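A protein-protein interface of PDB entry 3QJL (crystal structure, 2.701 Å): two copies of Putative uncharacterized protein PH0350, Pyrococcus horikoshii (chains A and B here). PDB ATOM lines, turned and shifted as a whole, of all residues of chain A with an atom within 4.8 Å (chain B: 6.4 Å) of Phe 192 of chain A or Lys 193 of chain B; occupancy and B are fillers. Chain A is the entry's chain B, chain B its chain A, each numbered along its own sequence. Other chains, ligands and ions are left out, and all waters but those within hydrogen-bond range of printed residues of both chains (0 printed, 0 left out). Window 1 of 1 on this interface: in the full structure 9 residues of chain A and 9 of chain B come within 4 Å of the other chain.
NZ of Lys 193 of chain B lies within hydrogen-bond range of O of Phe 192 of chain A, 3.3 Å away.
The backbone NH (N) of Leu 208 of chain B sits at hydrogen-bond distance from the backbone carbonyl oxygen (O) of Lys 193 of chain B (2.8 Å). N of Lys 193 of chain A sits at hydrogen-bond distance from O of Leu 208 of chain A.
Among the printed residues, pairs that only touch across the chains: Lys 193 of chain A with Phe 192 of chain B.
Phe 192 of chain A touches just one residue of chain B: Lys 193. Lys 193 of chain B touches just one residue of chain A: Phe 192. Of the printed residues of chain A, Phe 192 of chain B touches Lys 193 (3.4 Å). Of the printed residues of chain B, Lys 193 of chain A touches Phe 192 (3.4 Å). The nearest residue of chain A that does not touch Lys 193 of chain B is Lys 191 of chain A (4.3 Å).
Of the 11 printed residues of chain B, 2 touch a printed residue of chain A. Along chain B the printed residues that touch a printed residue of chain A span positions 192 to 193. Among the printed residues, no Asp or Glu carboxylate lies within 4 Å of a Lys or Arg side-chain nitrogen of the other chain.
Phe 192 of chain A touches Lys 193 of chain B, and with the chains exchanged Lys 193 of chain A touches Phe 192 of chain B. 9 positions are printed for both chains. Of the 2 pairs that touch across the chains among the printed residues, 2 have their exchanged pair printed and touching as well.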
ATOM      1  N   TYR A 154       2.322 -15.552  -6.425  1.00  0.00           N
ATOM      2  CA  TYR A 154       3.146 -14.424  -6.055  1.00  0.00           C
ATOM      3  C   TYR A 154       4.525 -14.644  -6.685  1.00  0.00           C
ATOM      4  O   TYR A 154       4.843 -15.760  -7.091  1.00  0.00           O
ATOM      5  CB  TYR A 154       3.309 -14.368  -4.545  1.00  0.00           C
ATOM      6  CG  TYR A 154       2.067 -14.447  -3.680  1.00  0.00           C
ATOM      7  CD1 TYR A 154       1.230 -13.352  -3.510  1.00  0.00           C
ATOM      8  CD2 TYR A 154       1.787 -15.592  -2.960  1.00  0.00           C
ATOM      9  CE1 TYR A 154       0.124 -13.423  -2.675  1.00  0.00           C
ATOM     10  CE2 TYR A 154       0.692 -15.662  -2.125  1.00  0.00           C
ATOM     11  CZ  TYR A 154      -0.129 -14.580  -1.986  1.00  0.00           C
ATOM     12  OH  TYR A 154      -1.210 -14.684  -1.147  1.00  0.00           O
ATOM     13  N   PRO A 155       5.363 -13.588  -6.746  1.00  0.00           N
ATOM     14  CA  PRO A 155       6.663 -13.660  -7.424  1.00  0.00           C
ATOM     15  C   PRO A 155       7.605 -14.735  -6.917  1.00  0.00           C
ATOM     16  O   PRO A 155       8.503 -15.119  -7.666  1.00  0.00           O
ATOM     17  CB  PRO A 155       7.255 -12.284  -7.170  1.00  0.00           C
ATOM     18  CG  PRO A 155       6.062 -11.405  -7.088  1.00  0.00           C
ATOM     19  CD  PRO A 155       5.067 -12.212  -6.310  1.00  0.00           C
ATOM     20  N   VAL A 189      11.548  -7.703  -7.723  1.00  0.00           N
ATOM     21  CA  VAL A 189      10.851  -7.166  -6.561  1.00  0.00           C
ATOM     22  C   VAL A 189      11.748  -6.397  -5.583  1.00  0.00           C
ATOM     23  O   VAL A 189      12.746  -6.919  -5.072  1.00  0.00           O
ATOM     24  CB  VAL A 189      10.161  -8.291  -5.777  1.00  0.00           C
ATOM     25  CG1 VAL A 189       9.397  -7.722  -4.583  1.00  0.00           C
ATOM     26  CG2 VAL A 189       9.253  -9.082  -6.686  1.00  0.00           C
ATOM     27  N   LEU A 190      11.355  -5.160  -5.311  1.00  0.00           N
ATOM     28  CA  LEU A 190      12.034  -4.320  -4.338  1.00  0.00           C
ATOM     29  C   LEU A 190      11.341  -4.373  -2.969  1.00  0.00           C
ATOM     30  O   LEU A 190      11.968  -4.701  -1.965  1.00  0.00           O
ATOM     31  CB  LEU A 190      12.147  -2.891  -4.861  1.00  0.00           C
ATOM     32  CG  LEU A 190      12.889  -2.859  -6.190  1.00  0.00           C
ATOM     33  CD1 LEU A 190      12.911  -1.464  -6.769  1.00  0.00           C
ATOM     34  CD2 LEU A 190      14.289  -3.408  -6.006  1.00  0.00           C
ATOM     35  N   LYS A 191      10.068  -3.994  -2.925  1.00  0.00           N
ATOM     36  CA  LYS A 191       9.293  -4.076  -1.692  1.00  0.00           C
ATOM     37  C   LYS A 191       8.042  -4.903  -1.964  1.00  0.00           C
ATOM     38  O   LYS A 191       7.368  -4.679  -2.959  1.00  0.00           O
ATOM     39  CB  LYS A 191       8.912  -2.672  -1.230  1.00  0.00           C
ATOM     40  CG  LYS A 191       8.517  -2.577   0.219  1.00  0.00           C
ATOM     41  CD  LYS A 191       8.023  -1.183   0.547  1.00  0.00           C
ATOM     42  CE  LYS A 191       7.647  -1.057   2.003  1.00  0.00           C
ATOM     43  NZ  LYS A 191       8.598  -0.167   2.718  1.00  0.00           N
ATOM     44  N   PHE A 192       7.738  -5.859  -1.089  1.00  0.00           N
ATOM     45  CA  PHE A 192       6.642  -6.796  -1.328  1.00  0.00           C
ATOM     46  C   PHE A 192       5.797  -7.148  -0.112  1.00  0.00           C
ATOM     47  O   PHE A 192       6.334  -7.571   0.912  1.00  0.00           O
ATOM     48  CB  PHE A 192       7.186  -8.105  -1.908  1.00  0.00           C
ATOM     49  CG  PHE A 192       6.175  -9.221  -1.922  1.00  0.00           C
ATOM     50  CD1 PHE A 192       5.194  -9.276  -2.903  1.00  0.00           C
ATOM     51  CD2 PHE A 192       6.197 -10.203  -0.950  1.00  0.00           C
ATOM     52  CE1 PHE A 192       4.256 -10.296  -2.915  1.00  0.00           C
ATOM     53  CE2 PHE A 192       5.271 -11.214  -0.948  1.00  0.00           C
ATOM     54  CZ  PHE A 192       4.293 -11.267  -1.937  1.00  0.00           C
ATOM     55  N   LYS A 193       4.475  -7.012  -0.240  1.00  0.00           N
ATOM     56  CA  LYS A 193       3.543  -7.527   0.769  1.00  0.00           C
ATOM     57  C   LYS A 193       2.333  -8.207   0.121  1.00  0.00           C
ATOM     58  O   LYS A 193       1.770  -7.686  -0.841  1.00  0.00           O
ATOM     59  CB  LYS A 193       3.056  -6.373   1.645  1.00  0.00           C
ATOM     60  CG  LYS A 193       2.108  -6.759   2.763  1.00  0.00           C
ATOM     61  CD  LYS A 193       1.295  -5.554   3.179  1.00  0.00           C
ATOM     62  CE  LYS A 193       1.455  -5.258   4.649  1.00  0.00           C
ATOM     63  NZ  LYS A 193       0.522  -4.172   5.050  1.00  0.00           N
ATOM     64  N   PRO A 194       1.916  -9.367   0.653  1.00  0.00           N
ATOM     65  CA  PRO A 194       0.740 -10.104   0.154  1.00  0.00           C
ATOM     66  C   PRO A 194      -0.577  -9.568   0.704  1.00  0.00           C
ATOM     67  O   PRO A 194      -0.615  -9.072   1.826  1.00  0.00           O
ATOM     68  CB  PRO A 194       0.979 -11.516   0.668  1.00  0.00           C
ATOM     69  CG  PRO A 194       1.734 -11.303   1.939  1.00  0.00           C
ATOM     70  CD  PRO A 194       2.608 -10.092   1.732  1.00  0.00           C
ATOM     71  N   SER A 207      -0.494  -9.148  -4.954  1.00  0.00           N
ATOM     72  CA  SER A 207       0.744  -8.560  -4.496  1.00  0.00           C
ATOM     73  C   SER A 207       0.678  -7.048  -4.424  1.00  0.00           C
ATOM     74  O   SER A 207       0.370  -6.403  -5.424  1.00  0.00           O
ATOM     75  CB  SER A 207       1.873  -8.980  -5.430  1.00  0.00           C
ATOM     76  OG  SER A 207       2.073 -10.379  -5.344  1.00  0.00           O
ATOM     77  N   LEU A 208       0.945  -6.497  -3.234  1.00  0.00           N
ATOM     78  CA  LEU A 208       1.195  -5.065  -3.062  1.00  0.00           C
ATOM     79  C   LEU A 208       2.694  -4.927  -3.080  1.00  0.00           C
ATOM     80  O   LEU A 208       3.392  -5.527  -2.253  1.00  0.00           O
ATOM     81  CB  LEU A 208       0.653  -4.566  -1.733  1.00  0.00           C
ATOM     82  CG  LEU A 208      -0.853  -4.379  -1.640  1.00  0.00           C
ATOM     83  CD1 LEU A 208      -1.281  -4.212  -0.201  1.00  0.00           C
ATOM     84  CD2 LEU A 208      -1.252  -3.175  -2.460  1.00  0.00           C
ATOM     85  N   MET A 209       3.223  -4.185  -4.037  1.00  0.00           N
ATOM     86  CA  MET A 209       4.666  -4.221  -4.197  1.00  0.00           C
ATOM     87  C   MET A 209       5.228  -3.029  -4.953  1.00  0.00           C
ATOM     88  O   MET A 209       4.503  -2.275  -5.615  1.00  0.00           O
ATOM     89  CB  MET A 209       5.088  -5.537  -4.868  1.00  0.00           C
ATOM     90  CG  MET A 209       4.459  -5.703  -6.255  1.00  0.00           C
ATOM     91  SD  MET A 209       4.997  -7.141  -7.180  1.00  0.00           S
ATOM     92  CE  MET A 209       6.758  -7.012  -6.880  1.00  0.00           C
ATOM     93  N   TYR B 154       3.248 -15.900  14.390  1.00  0.00           N
ATOM     94  CA  TYR B 154       2.832 -14.539  14.101  1.00  0.00           C
ATOM     95  C   TYR B 154       1.482 -14.320  14.762  1.00  0.00           C
ATOM     96  O   TYR B 154       0.820 -15.272  15.166  1.00  0.00           O
ATOM     97  CB  TYR B 154       2.667 -14.315  12.611  1.00  0.00           C
ATOM     98  CG  TYR B 154       3.816 -14.716  11.721  1.00  0.00           C
ATOM     99  CD1 TYR B 154       4.890 -13.865  11.517  1.00  0.00           C
ATOM    100  CD2 TYR B 154       3.789 -15.917  11.026  1.00  0.00           C
ATOM    101  CE1 TYR B 154       5.920 -14.215  10.669  1.00  0.00           C
ATOM    102  CE2 TYR B 154       4.814 -16.276  10.177  1.00  0.00           C
ATOM    103  CZ  TYR B 154       5.874 -15.424   9.998  1.00  0.00           C
ATOM    104  OH  TYR B 154       6.890 -15.782   9.146  1.00  0.00           O
ATOM    105  N   VAL B 189      -3.272  -6.410  16.260  1.00  0.00           N
ATOM    106  CA  VAL B 189      -2.483  -6.004  15.117  1.00  0.00           C
ATOM    107  C   VAL B 189      -3.215  -4.939  14.314  1.00  0.00           C
ATOM    108  O   VAL B 189      -4.435  -4.968  14.194  1.00  0.00           O
ATOM    109  CB  VAL B 189      -2.220  -7.215  14.232  1.00  0.00           C
ATOM    110  CG1 VAL B 189      -1.523  -6.815  12.957  1.00  0.00           C
ATOM    111  CG2 VAL B 189      -1.411  -8.214  14.988  1.00  0.00           C
ATOM    112  N   LYS B 191      -1.122  -2.900  11.522  1.00  0.00           N
ATOM    113  CA  LYS B 191      -0.431  -3.108  10.257  1.00  0.00           C
ATOM    114  C   LYS B 191       0.523  -4.270  10.490  1.00  0.00           C
ATOM    115  O   LYS B 191       1.247  -4.281  11.474  1.00  0.00           O
ATOM    116  CB  LYS B 191       0.343  -1.844   9.890  1.00  0.00           C
ATOM    117  CG  LYS B 191       1.001  -1.833   8.534  1.00  0.00           C
ATOM    118  CD  LYS B 191       1.607  -0.457   8.280  1.00  0.00           C
ATOM    119  CE  LYS B 191       2.118  -0.288   6.859  1.00  0.00           C
ATOM    120  NZ  LYS B 191       0.992  -0.026   5.900  1.00  0.00           N
ATOM    121  N   PHE B 192       0.468  -5.294   9.644  1.00  0.00           N
ATOM    122  CA  PHE B 192       1.293  -6.478   9.880  1.00  0.00           C
ATOM    123  C   PHE B 192       2.071  -7.005   8.679  1.00  0.00           C
ATOM    124  O   PHE B 192       1.561  -7.048   7.561  1.00  0.00           O
ATOM    125  CB  PHE B 192       0.448  -7.610  10.471  1.00  0.00           C
ATOM    126  CG  PHE B 192       1.124  -8.950  10.429  1.00  0.00           C
ATOM    127  CD1 PHE B 192       1.984  -9.339  11.442  1.00  0.00           C
ATOM    128  CD2 PHE B 192       0.906  -9.818   9.374  1.00  0.00           C
ATOM    129  CE1 PHE B 192       2.609 -10.570  11.405  1.00  0.00           C
ATOM    130  CE2 PHE B 192       1.528 -11.051   9.331  1.00  0.00           C
ATOM    131  CZ  PHE B 192       2.381 -11.426  10.348  1.00  0.00           C
ATOM    132  N   LYS B 193       3.312  -7.410   8.930  1.00  0.00           N
ATOM    133  CA  LYS B 193       4.147  -8.031   7.910  1.00  0.00           C
ATOM    134  C   LYS B 193       5.071  -9.083   8.525  1.00  0.00           C
ATOM    135  O   LYS B 193       5.490  -8.955   9.674  1.00  0.00           O
ATOM    136  CB  LYS B 193       4.972  -6.971   7.180  1.00  0.00           C
ATOM    137  CG  LYS B 193       5.586  -7.450   5.877  1.00  0.00           C
ATOM    138  CD  LYS B 193       5.930  -6.282   4.968  1.00  0.00           C
ATOM    139  CE  LYS B 193       7.310  -6.446   4.355  1.00  0.00           C
ATOM    140  NZ  LYS B 193       7.514  -5.533   3.198  1.00  0.00           N
ATOM    141  N   PRO B 194       5.400 -10.110   7.748  1.00  0.00           N
ATOM    142  CA  PRO B 194       6.371 -11.136   8.176  1.00  0.00           C
ATOM    143  C   PRO B 194       7.797 -10.871   7.651  1.00  0.00           C
ATOM    144  O   PRO B 194       7.975 -10.302   6.572  1.00  0.00           O
ATOM    145  CB  PRO B 194       5.832 -12.412   7.498  1.00  0.00           C
ATOM    146  CG  PRO B 194       5.258 -11.897   6.233  1.00  0.00           C
ATOM    147  CD  PRO B 194       4.593 -10.594   6.613  1.00  0.00           C
ATOM    148  N   THR B 195       8.820 -11.293   8.380  1.00  0.00           N
ATOM    149  CA  THR B 195      10.170 -11.109   7.882  1.00  0.00           C
ATOM    150  C   THR B 195      10.961 -12.349   8.264  1.00  0.00           C
ATOM    151  O   THR B 195      10.653 -12.999   9.270  1.00  0.00           O
ATOM    152  CB  THR B 195      10.779  -9.824   8.488  1.00  0.00           C
ATOM    153  OG1 THR B 195      11.892  -9.374   7.707  1.00  0.00           O
ATOM    154  CG2 THR B 195      11.200 -10.063   9.925  1.00  0.00           C
ATOM    155  N   GLY B 206       9.846 -13.352  12.034  1.00  0.00           N
ATOM    156  CA  GLY B 206       9.188 -12.500  13.006  1.00  0.00           C
ATOM    157  C   GLY B 206       8.253 -11.512  12.347  1.00  0.00           C
ATOM    158  O   GLY B 206       8.080 -11.525  11.129  1.00  0.00           O
ATOM    159  N   SER B 207       7.654 -10.647  13.157  1.00  0.00           N
ATOM    160  CA  SER B 207       6.670  -9.702  12.657  1.00  0.00           C
ATOM    161  C   SER B 207       7.185  -8.264  12.701  1.00  0.00           C
ATOM    162  O   SER B 207       7.731  -7.825  13.709  1.00  0.00           O
ATOM    163  CB  SER B 207       5.382  -9.817  13.477  1.00  0.00           C
ATOM    164  OG  SER B 207       5.248 -11.120  14.021  1.00  0.00           O
ATOM    165  N   LEU B 208       7.029  -7.545  11.595  1.00  0.00           N
ATOM    166  CA  LEU B 208       7.149  -6.103  11.602  1.00  0.00           C
ATOM    167  C   LEU B 208       5.735  -5.567  11.574  1.00  0.00           C
ATOM    168  O   LEU B 208       5.048  -5.691  10.572  1.00  0.00           O
ATOM    169  CB  LEU B 208       7.877  -5.614  10.365  1.00  0.00           C
ATOM    170  CG  LEU B 208       9.239  -6.210  10.084  1.00  0.00           C
ATOM    171  CD1 LEU B 208       9.690  -5.775   8.700  1.00  0.00           C
ATOM    172  CD2 LEU B 208      10.226  -5.774  11.141  1.00  0.00           C
ATOM    173  N   MET B 209       5.293  -4.953  12.656  1.00  0.00           N
ATOM    174  CA  MET B 209       3.891  -4.626  12.773  1.00  0.00           C
ATOM    175  C   MET B 209       3.680  -3.334  13.541  1.00  0.00           C
ATOM    176  O   MET B 209       4.555  -2.884  14.294  1.00  0.00           O
ATOM    177  CB  MET B 209       3.183  -5.764  13.500  1.00  0.00           C
ATOM    178  CG  MET B 209       3.786  -6.053  14.851  1.00  0.00           C
ATOM    179  SD  MET B 209       3.082  -7.477  15.687  1.00  0.00           S
ATOM    180  CE  MET B 209       1.423  -7.336  15.050  1.00  0.00           C
